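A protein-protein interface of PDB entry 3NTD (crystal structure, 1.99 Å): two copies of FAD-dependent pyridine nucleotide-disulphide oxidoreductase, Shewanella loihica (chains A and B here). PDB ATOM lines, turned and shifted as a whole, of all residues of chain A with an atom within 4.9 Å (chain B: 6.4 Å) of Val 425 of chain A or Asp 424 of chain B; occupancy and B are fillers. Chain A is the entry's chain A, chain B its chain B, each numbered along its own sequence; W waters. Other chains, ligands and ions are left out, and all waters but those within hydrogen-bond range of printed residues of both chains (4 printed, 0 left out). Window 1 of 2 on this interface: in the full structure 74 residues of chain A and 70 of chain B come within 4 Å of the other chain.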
ATOM      1  N   LYS A 421      25.060   1.993 -15.186  1.00  0.00           N
ATOM      2  CA  LYS A 421      24.632   3.400 -15.208  1.00  0.00           C
ATOM      3  C   LYS A 421      23.121   3.579 -15.403  1.00  0.00           C
ATOM      4  O   LYS A 421      22.491   4.435 -14.782  1.00  0.00           O
ATOM      5  CB  LYS A 421      25.365   4.077 -16.390  1.00  0.00           C
ATOM      6  CG  LYS A 421      24.862   5.550 -16.563  1.00  0.00           C
ATOM      7  CD  LYS A 421      25.745   6.529 -17.521  1.00  0.00           C
ATOM      8  CE  LYS A 421      25.706   6.066 -18.959  1.00  0.00           C
ATOM      9  NZ  LYS A 421      26.569   6.731 -19.939  1.00  0.00           N
ATOM     10  N   ARG A 422      22.545   2.813 -16.335  1.00  0.00           N
ATOM     11  CA  ARG A 422      21.106   2.836 -16.589  1.00  0.00           C
ATOM     12  C   ARG A 422      20.331   2.282 -15.352  1.00  0.00           C
ATOM     13  O   ARG A 422      19.345   2.825 -14.979  1.00  0.00           O
ATOM     14  CB  ARG A 422      20.790   2.023 -17.887  1.00  0.00           C
ATOM     15  CG  ARG A 422      20.960   2.808 -19.215  1.00  0.00           C
ATOM     16  CD  ARG A 422      22.035   3.844 -19.132  1.00  0.00           C
ATOM     17  NE  ARG A 422      22.339   4.605 -20.352  1.00  0.00           N
ATOM     18  CZ  ARG A 422      23.382   4.360 -21.143  1.00  0.00           C
ATOM     19  NH1 ARG A 422      24.202   3.360 -20.889  1.00  0.00           N
ATOM     20  NH2 ARG A 422      23.620   5.173 -22.204  1.00  0.00           N
ATOM     21  N   ILE A 423      20.810   1.274 -14.652  1.00  0.00           N
ATOM     22  CA  ILE A 423      20.104   0.756 -13.495  1.00  0.00           C
ATOM     23  C   ILE A 423      20.119   1.828 -12.330  1.00  0.00           C
ATOM     24  O   ILE A 423      19.087   2.202 -11.792  1.00  0.00           O
ATOM     25  CB  ILE A 423      20.680  -0.570 -13.083  1.00  0.00           C
ATOM     26  CG1 ILE A 423      20.363  -1.647 -14.150  1.00  0.00           C
ATOM     27  CG2 ILE A 423      20.063  -1.089 -11.750  1.00  0.00           C
ATOM     28  CD1 ILE A 423      18.921  -1.430 -14.583  1.00  0.00           C
ATOM     29  N   ASP A 424      21.266   2.434 -12.102  1.00  0.00           N
ATOM     30  CA  ASP A 424      21.417   3.511 -11.103  1.00  0.00           C
ATOM     31  C   ASP A 424      20.503   4.678 -11.325  1.00  0.00           C
ATOM     32  O   ASP A 424      19.849   5.168 -10.355  1.00  0.00           O
ATOM     33  CB  ASP A 424      22.886   3.980 -11.087  1.00  0.00           C
ATOM     34  CG  ASP A 424      23.835   2.963 -10.381  1.00  0.00           C
ATOM     35  OD1 ASP A 424      23.364   1.838 -10.093  1.00  0.00           O
ATOM     36  OD2 ASP A 424      25.018   3.283 -10.096  1.00  0.00           O
ATOM     37  N   VAL A 425      20.558   5.231 -12.546  1.00  0.00           N
ATOM     38  CA  VAL A 425      19.595   6.290 -13.020  1.00  0.00           C
ATOM     39  C   VAL A 425      18.203   5.822 -12.630  1.00  0.00           C
ATOM     40  O   VAL A 425      17.489   6.531 -11.992  1.00  0.00           O
ATOM     41  CB  VAL A 425      19.626   6.590 -14.505  1.00  0.00           C
ATOM     42  CG1 VAL A 425      18.349   7.457 -15.059  1.00  0.00           C
ATOM     43  CG2 VAL A 425      20.964   7.323 -15.003  1.00  0.00           C
ATOM     44  N   MET A 426      17.785   4.670 -13.109  1.00  0.00           N
ATOM     45  CA  MET A 426      16.380   4.201 -12.747  1.00  0.00           C
ATOM     46  C   MET A 426      16.211   4.050 -11.255  1.00  0.00           C
ATOM     47  O   MET A 426      15.115   4.288 -10.711  1.00  0.00           O
ATOM     48  CB  MET A 426      16.169   2.833 -13.421  1.00  0.00           C
ATOM     49  CG  MET A 426      15.943   2.951 -14.919  1.00  0.00           C
ATOM     50  SD  MET A 426      14.790   4.267 -15.425  1.00  0.00           S
ATOM     51  CE  MET A 426      13.397   3.644 -14.469  1.00  0.00           C
ATOM     52  N   ALA A 427      17.242   3.587 -10.527  1.00  0.00           N
ATOM     53  CA  ALA A 427      17.040   3.403  -9.117  1.00  0.00           C
ATOM     54  C   ALA A 427      16.842   4.706  -8.381  1.00  0.00           C
ATOM     55  O   ALA A 427      16.042   4.777  -7.447  1.00  0.00           O
ATOM     56  CB  ALA A 427      18.233   2.591  -8.448  1.00  0.00           C
ATOM     57  N   VAL A 428      17.556   5.747  -8.813  1.00  0.00           N
ATOM     58  CA  VAL A 428      17.366   7.059  -8.190  1.00  0.00           C
ATOM     59  C   VAL A 428      16.030   7.586  -8.661  1.00  0.00           C
ATOM     60  O   VAL A 428      15.166   8.091  -7.875  1.00  0.00           O
ATOM     61  CB  VAL A 428      18.485   8.055  -8.754  1.00  0.00           C
ATOM     62  CG1 VAL A 428      18.158   9.528  -8.238  1.00  0.00           C
ATOM     63  CG2 VAL A 428      19.846   7.547  -8.506  1.00  0.00           C
ATOM     64  N   ALA A 429      15.745   7.454  -9.965  1.00  0.00           N
ATOM     65  CA  ALA A 429      14.378   8.024 -10.388  1.00  0.00           C
ATOM     66  C   ALA A 429      13.192   7.365  -9.663  1.00  0.00           C
ATOM     67  O   ALA A 429      12.205   8.016  -9.356  1.00  0.00           O
ATOM     68  CB  ALA A 429      14.131   7.873 -11.867  1.00  0.00           C
ATOM     69  N   LEU A 442      14.613  14.012 -18.444  1.00  0.00           N
ATOM     70  CA  LEU A 442      16.003  13.760 -17.963  1.00  0.00           C
ATOM     71  C   LEU A 442      17.056  14.358 -18.914  1.00  0.00           C
ATOM     72  O   LEU A 442      16.972  14.238 -20.157  1.00  0.00           O
ATOM     73  CB  LEU A 442      16.297  12.323 -17.577  1.00  0.00           C
ATOM     74  CG  LEU A 442      15.583  11.777 -16.349  1.00  0.00           C
ATOM     75  CD1 LEU A 442      15.941  10.303 -16.158  1.00  0.00           C
ATOM     76  CD2 LEU A 442      15.893  12.596 -15.039  1.00  0.00           C
ATOM     77  N   LEU A 444      20.805  14.131 -19.289  1.00  0.00           N
ATOM     78  CA  LEU A 444      21.950  13.308 -18.919  1.00  0.00           C
ATOM     79  C   LEU A 444      23.245  13.745 -19.637  1.00  0.00           C
ATOM     80  O   LEU A 444      23.212  14.554 -20.536  1.00  0.00           O
ATOM     81  CB  LEU A 444      21.610  11.789 -19.103  1.00  0.00           C
ATOM     82  CG  LEU A 444      20.377  11.286 -18.272  1.00  0.00           C
ATOM     83  CD1 LEU A 444      20.275   9.696 -18.372  1.00  0.00           C
ATOM     84  CD2 LEU A 444      20.603  11.670 -16.814  1.00  0.00           C
ATOM     85  N   SER A 445      24.379  13.200 -19.226  1.00  0.00           N
ATOM     86  CA  SER A 445      25.720  13.557 -19.772  1.00  0.00           C
ATOM     87  C   SER A 445      25.879  13.032 -21.219  1.00  0.00           C
ATOM     88  O   SER A 445      25.973  11.805 -21.390  1.00  0.00           O
ATOM     89  CB  SER A 445      26.767  12.797 -18.967  1.00  0.00           C
ATOM     90  OG  SER A 445      26.757  13.202 -17.594  1.00  0.00           O
ATOM     91  N   ILE A 457      17.494   5.801 -21.487  1.00  0.00           N
ATOM     92  CA  ILE A 457      16.415   6.210 -20.555  1.00  0.00           C
ATOM     93  C   ILE A 457      15.437   7.203 -21.141  1.00  0.00           C
ATOM     94  O   ILE A 457      14.246   7.068 -20.876  1.00  0.00           O
ATOM     95  CB  ILE A 457      16.985   6.779 -19.169  1.00  0.00           C
ATOM     96  CG1 ILE A 457      18.081   5.846 -18.580  1.00  0.00           C
ATOM     97  CG2 ILE A 457      15.896   7.024 -18.126  1.00  0.00           C
ATOM     98  CD1 ILE A 457      17.615   4.513 -18.261  1.00  0.00           C
ATOM     99  N   THR B 348      23.996  19.748 -17.772  1.00  0.00           N
ATOM    100  CA  THR B 348      24.665  18.490 -17.636  1.00  0.00           C
ATOM    101  C   THR B 348      25.607  18.394 -18.846  1.00  0.00           C
ATOM    102  O   THR B 348      25.159  18.509 -19.935  1.00  0.00           O
ATOM    103  CB  THR B 348      23.614  17.296 -17.625  1.00  0.00           C
ATOM    104  OG1 THR B 348      22.629  17.589 -16.658  1.00  0.00           O
ATOM    105  CG2 THR B 348      24.210  15.995 -17.247  1.00  0.00           C
ATOM    106  N   ILE B 419      32.647   8.377 -14.459  1.00  0.00           N
ATOM    107  CA  ILE B 419      32.306   9.805 -14.279  1.00  0.00           C
ATOM    108  C   ILE B 419      30.911  10.094 -14.856  1.00  0.00           C
ATOM    109  O   ILE B 419      30.062  10.629 -14.141  1.00  0.00           O
ATOM    110  CB  ILE B 419      33.374  10.742 -14.928  1.00  0.00           C
ATOM    111  CG1 ILE B 419      34.780  10.492 -14.311  1.00  0.00           C
ATOM    112  CG2 ILE B 419      32.958  12.280 -14.814  1.00  0.00           C
ATOM    113  CD1 ILE B 419      34.776  10.422 -12.832  1.00  0.00           C
ATOM    114  N   ASP B 420      30.657   9.509 -16.046  1.00  0.00           N
ATOM    115  CA  ASP B 420      29.283   9.585 -16.617  1.00  0.00           C
ATOM    116  C   ASP B 420      28.229   9.006 -15.725  1.00  0.00           C
ATOM    117  O   ASP B 420      27.171   9.581 -15.604  1.00  0.00           O
ATOM    118  CB  ASP B 420      29.181   9.003 -18.028  1.00  0.00           C
ATOM    119  CG  ASP B 420      29.628   7.520 -18.138  1.00  0.00           C
ATOM    120  OD1 ASP B 420      30.450   7.085 -17.336  1.00  0.00           O
ATOM    121  OD2 ASP B 420      29.031   6.787 -18.993  1.00  0.00           O
ATOM    122  N   LYS B 421      28.551   7.956 -15.000  1.00  0.00           N
ATOM    123  CA  LYS B 421      27.511   7.363 -14.138  1.00  0.00           C
ATOM    124  C   LYS B 421      27.132   8.335 -12.960  1.00  0.00           C
ATOM    125  O   LYS B 421      25.958   8.627 -12.715  1.00  0.00           O
ATOM    126  CB  LYS B 421      27.971   5.982 -13.661  1.00  0.00           C
ATOM    127  CG  LYS B 421      26.836   5.325 -12.712  1.00  0.00           C
ATOM    128  CD  LYS B 421      27.133   3.931 -12.330  1.00  0.00           C
ATOM    129  CE  LYS B 421      28.555   3.750 -11.694  1.00  0.00           C
ATOM    130  NZ  LYS B 421      28.607   2.325 -11.474  1.00  0.00           N
ATOM    131  N   ARG B 422      28.145   8.839 -12.225  1.00  0.00           N
ATOM    132  CA  ARG B 422      27.871   9.758 -11.125  1.00  0.00           C
ATOM    133  C   ARG B 422      27.243  11.102 -11.454  1.00  0.00           C
ATOM    134  O   ARG B 422      26.455  11.574 -10.671  1.00  0.00           O
ATOM    135  CB  ARG B 422      29.192  10.015 -10.343  1.00  0.00           C
ATOM    136  CG  ARG B 422      29.550   8.970  -9.409  1.00  0.00           C
ATOM    137  CD  ARG B 422      29.137   7.482  -9.881  1.00  0.00           C
ATOM    138  NE  ARG B 422      29.643   6.370  -9.096  1.00  0.00           N
ATOM    139  CZ  ARG B 422      30.605   5.481  -9.454  1.00  0.00           C
ATOM    140  NH1 ARG B 422      31.315   5.562 -10.552  1.00  0.00           N
ATOM    141  NH2 ARG B 422      30.864   4.453  -8.678  1.00  0.00           N
ATOM    142  N   ILE B 423      27.613  11.722 -12.571  1.00  0.00           N
ATOM    143  CA  ILE B 423      26.946  12.876 -13.096  1.00  0.00           C
ATOM    144  C   ILE B 423      25.502  12.575 -13.497  1.00  0.00           C
ATOM    145  O   ILE B 423      24.566  13.320 -13.108  1.00  0.00           O
ATOM    146  CB  ILE B 423      27.769  13.535 -14.187  1.00  0.00           C
ATOM    147  CG1 ILE B 423      29.127  13.935 -13.582  1.00  0.00           C
ATOM    148  CG2 ILE B 423      27.123  14.719 -14.685  1.00  0.00           C
ATOM    149  CD1 ILE B 423      28.965  14.982 -12.492  1.00  0.00           C
ATOM    150  N   ASP B 424      25.278  11.438 -14.116  1.00  0.00           N
ATOM    151  CA  ASP B 424      23.818  11.102 -14.448  1.00  0.00           C
ATOM    152  C   ASP B 424      22.974  10.930 -13.198  1.00  0.00           C
ATOM    153  O   ASP B 424      21.858  11.484 -13.146  1.00  0.00           O
ATOM    154  CB  ASP B 424      23.656   9.895 -15.418  1.00  0.00           C
ATOM    155  CG  ASP B 424      24.209  10.230 -16.802  1.00  0.00           C
ATOM    156  OD1 ASP B 424      24.658  11.410 -17.024  1.00  0.00           O
ATOM    157  OD2 ASP B 424      24.176   9.361 -17.689  1.00  0.00           O
ATOM    158  N   VAL B 425      23.469  10.149 -12.224  1.00  0.00           N
ATOM    159  CA  VAL B 425      22.759   9.958 -10.960  1.00  0.00           C
ATOM    160  C   VAL B 425      22.450  11.312 -10.287  1.00  0.00           C
ATOM    161  O   VAL B 425      21.328  11.551  -9.887  1.00  0.00           O
ATOM    162  CB  VAL B 425      23.563   8.974  -9.970  1.00  0.00           C
ATOM    163  CG1 VAL B 425      23.227   9.243  -8.512  1.00  0.00           C
ATOM    164  CG2 VAL B 425      23.303   7.509 -10.333  1.00  0.00           C
ATOM    165  N   MET B 426      23.454  12.194 -10.180  1.00  0.00           N
ATOM    166  CA  MET B 426      23.212  13.593  -9.610  1.00  0.00           C
ATOM    167  C   MET B 426      22.257  14.472 -10.443  1.00  0.00           C
ATOM    168  O   MET B 426      21.535  15.323  -9.946  1.00  0.00           O
ATOM    169  CB  MET B 426      24.586  14.337  -9.513  1.00  0.00           C
ATOM    170  CG  MET B 426      25.423  13.702  -8.286  1.00  0.00           C
ATOM    171  SD  MET B 426      24.596  13.593  -6.755  1.00  0.00           S
ATOM    172  CE  MET B 426      23.892  15.263  -6.583  1.00  0.00           C
ATOM    173  N   ALA B 427      22.218  14.256 -11.735  1.00  0.00           N
ATOM    174  CA  ALA B 427      21.348  15.102 -12.570  1.00  0.00           C
ATOM    175  C   ALA B 427      19.923  14.620 -12.300  1.00  0.00           C
ATOM    176  O   ALA B 427      18.934  15.429 -12.126  1.00  0.00           O
ATOM    177  CB  ALA B 427      21.737  14.937 -14.085  1.00  0.00           C
ATOM    178  N   VAL B 428      19.769  13.302 -12.271  1.00  0.00           N
ATOM    179  CA  VAL B 428      18.467  12.724 -11.898  1.00  0.00           C
ATOM    180  C   VAL B 428      18.045  13.188 -10.497  1.00  0.00           C
ATOM    181  O   VAL B 428      16.912  13.633 -10.223  1.00  0.00           O
ATOM    182  CB  VAL B 428      18.411  11.142 -12.049  1.00  0.00           C
ATOM    183  CG1 VAL B 428      16.996  10.647 -11.715  1.00  0.00           C
ATOM    184  CG2 VAL B 428      18.734  10.754 -13.520  1.00  0.00           C
ATOM    185  N   ALA B 429      18.955  13.130  -9.536  1.00  0.00           N
ATOM    186  CA  ALA B 429      18.497  13.487  -8.190  1.00  0.00           C
ATOM    187  C   ALA B 429      18.088  14.928  -8.031  1.00  0.00           C
ATOM    188  O   ALA B 429      17.108  15.233  -7.391  1.00  0.00           O
ATOM    189  CB  ALA B 429      19.690  13.102  -7.134  1.00  0.00           C
ATOM    190  N   LEU B 444      22.208   1.788  -4.956  1.00  0.00           N
ATOM    191  CA  LEU B 444      22.650   1.781  -6.325  1.00  0.00           C
ATOM    192  C   LEU B 444      23.227   0.398  -6.641  1.00  0.00           C
ATOM    193  O   LEU B 444      23.284  -0.448  -5.782  1.00  0.00           O
ATOM    194  CB  LEU B 444      23.706   2.889  -6.661  1.00  0.00           C
ATOM    195  CG  LEU B 444      23.258   4.327  -6.381  1.00  0.00           C
ATOM    196  CD1 LEU B 444      24.380   5.315  -6.797  1.00  0.00           C
ATOM    197  CD2 LEU B 444      21.895   4.647  -7.153  1.00  0.00           C
HETATM  198  O   HOH W   1      22.715   7.536 -18.817  1.00  0.00           O
HETATM  199  O   HOH W   2      26.704   1.331  -9.484  1.00  0.00           O
HETATM  200  O   HOH W   3      25.182   9.508 -19.951  1.00  0.00           O
HETATM  201  O   HOH W   4      26.732   5.286  -9.078  1.00  0.00           O
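The side-chain carboxylate (OD2) of Asp 420 of chain B lies within salt-bridge range of the side-chain amino group (NZ) of Lys 421 of chain A.
The side-chain carboxylate of Asp 424 of chain A lies within salt-bridge range of the side-chain amino group of Lys 421 of chain B (3.96 Å).
The side-chain hydroxyl (OG) of Ser 445 of chain A lies within hydrogen-bond range of the side-chain carboxylate (OD1) of Asp 424 of chain B, 2.8 Å away.
Of chain B, only Asp 424 and Val 428 come within 4 Å of Val 425 of chain A.
Of chain A, only Lys 421 (3.2 Å), Val 425 (3.7 Å), Leu 444 (3.7 Å) and Ser 445 (2.8 Å) come within 4 Å of Asp 424 of chain B.
Of the printed residues of chain B, Ser 445 of chain A touches Thr 348 (3.4 Å), Ile 423 (3.3 Å) and Asp 424 (2.8 Å).
Of the printed residues of chain B, Asp 424 of chain A touches Lys 421 (3.1 Å), Val 425 (3.6 Å) and Leu 444 (3.6 Å).
Met 426 of chain A touches none of the printed residues of chain B.
The nearest residue of chain B that does not touch Val 425 of chain A is Val 425 of chain B (4.2 Å).
The nearest printed residue of chain A that does not touch Asp 424 of chain B is Arg 422 of chain A (5.8 Å).
The nearest printed residue of chain A that does not touch Ala 429 of chain B is Leu 442 of chain A (6.3 Å).
Water W3 lies within hydrogen-bond range of OD2 of Asp 424 of chain B (2.5 Å), O of Ser 445 of chain A (2.8 Å) and NZ of Lys 421 of chain A (3.1 Å).
Water W1 lies within hydrogen-bond range of the side-chain carboxylate of Asp 424 of chain B (2.6 Å) and the guanidinium group of Arg 422 of chain A (3.3 Å).
Water W2 lies within hydrogen-bond range of the side-chain carboxylate of Asp 424 of chain A (2.7 Å) and the side-chain amino group of Lys 421 of chain B (2.9 Å).
Water W4 bridges the side-chain carboxylate (OD2) of Asp 424 of chain A (2.8 Å) and the guanidinium group (NE) of Arg 422 of chain B (3.1 Å).
Lys 421 of chain A touches Asp 424 of chain B, and with the chains exchanged Asp 424 of chain A touches Lys 421 of chain B.
Asp 424 of chain A touches Val 425 of chain B, and with the chains exchanged Val 425 of chain A touches Asp 424 of chain B.
Val 428 of chain B touches its own counterpart, Val 428 of chain A.
Val 428 of chain A touches Ala 429 of chain B, and with the chains exchanged Ala 429 of chain A touches Val 428 of chain B.
Of the 20 pairs that touch across the chains among the printed residues, 14 have their exchanged pair printed and touching as well.
Printed residues of chain A that touch a printed residue of chain B: Lys 421, Asp 424, Val 425, Val 428, Ala 429, Leu 442, Leu 444 and Ser 445.
Hydrophobic or aromatic side chains of chain A that line the printed part of chain B: Val 425, Val 428, Ala 429, Leu 442 and Leu 444.
Hydrophobic or aromatic side chains of chain B that line the printed part of chain A: Ile 423, Val 425, Val 428 and Leu 444.
Among the printed residues, 20 pairs touch across the chains.
Among the printed residues, pairs that only touch across the chains: Lys 421 of chain A with Asp 424 of chain B (3.2 Å), Ser 445 of chain A with Ile 423 of chain B (3.3 Å), Leu 444 of chain A with Thr 348 of chain B (3.4 Å), Ser 445 of chain A with Thr 348 of chain B (3.4 Å), Asp 424 of chain A with Leu 444 of chain B (3.6 Å), Asp 424 of chain A with Val 425 of chain B (3.6 Å), Val 425 of chain A with Val 428 of chain B (3.7 Å), Leu 444 of chain A with Asp 424 of chain B (3.7 Å), Leu 442 of chain A with Val 428 of chain B (3.7 Å), Val 425 of chain A with Asp 424 of chain B (3.7 Å), Val 428 of chain A with Val 425 of chain B (3.8 Å), Val 428 of chain A with Leu 444 of chain B (3.8 Å), Val 428 of chain A with Val 428 of chain B (3.8 Å), Lys 421 of chain A with Lys 421 of chain B (3.8 Å), Ala 429 of chain A with Val 428 of chain B (3.9 Å), Leu 444 of chain A with Val 428 of chain B (3.9 Å) and Val 428 of chain A with Ala 429 of chain B (3.9 Å).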
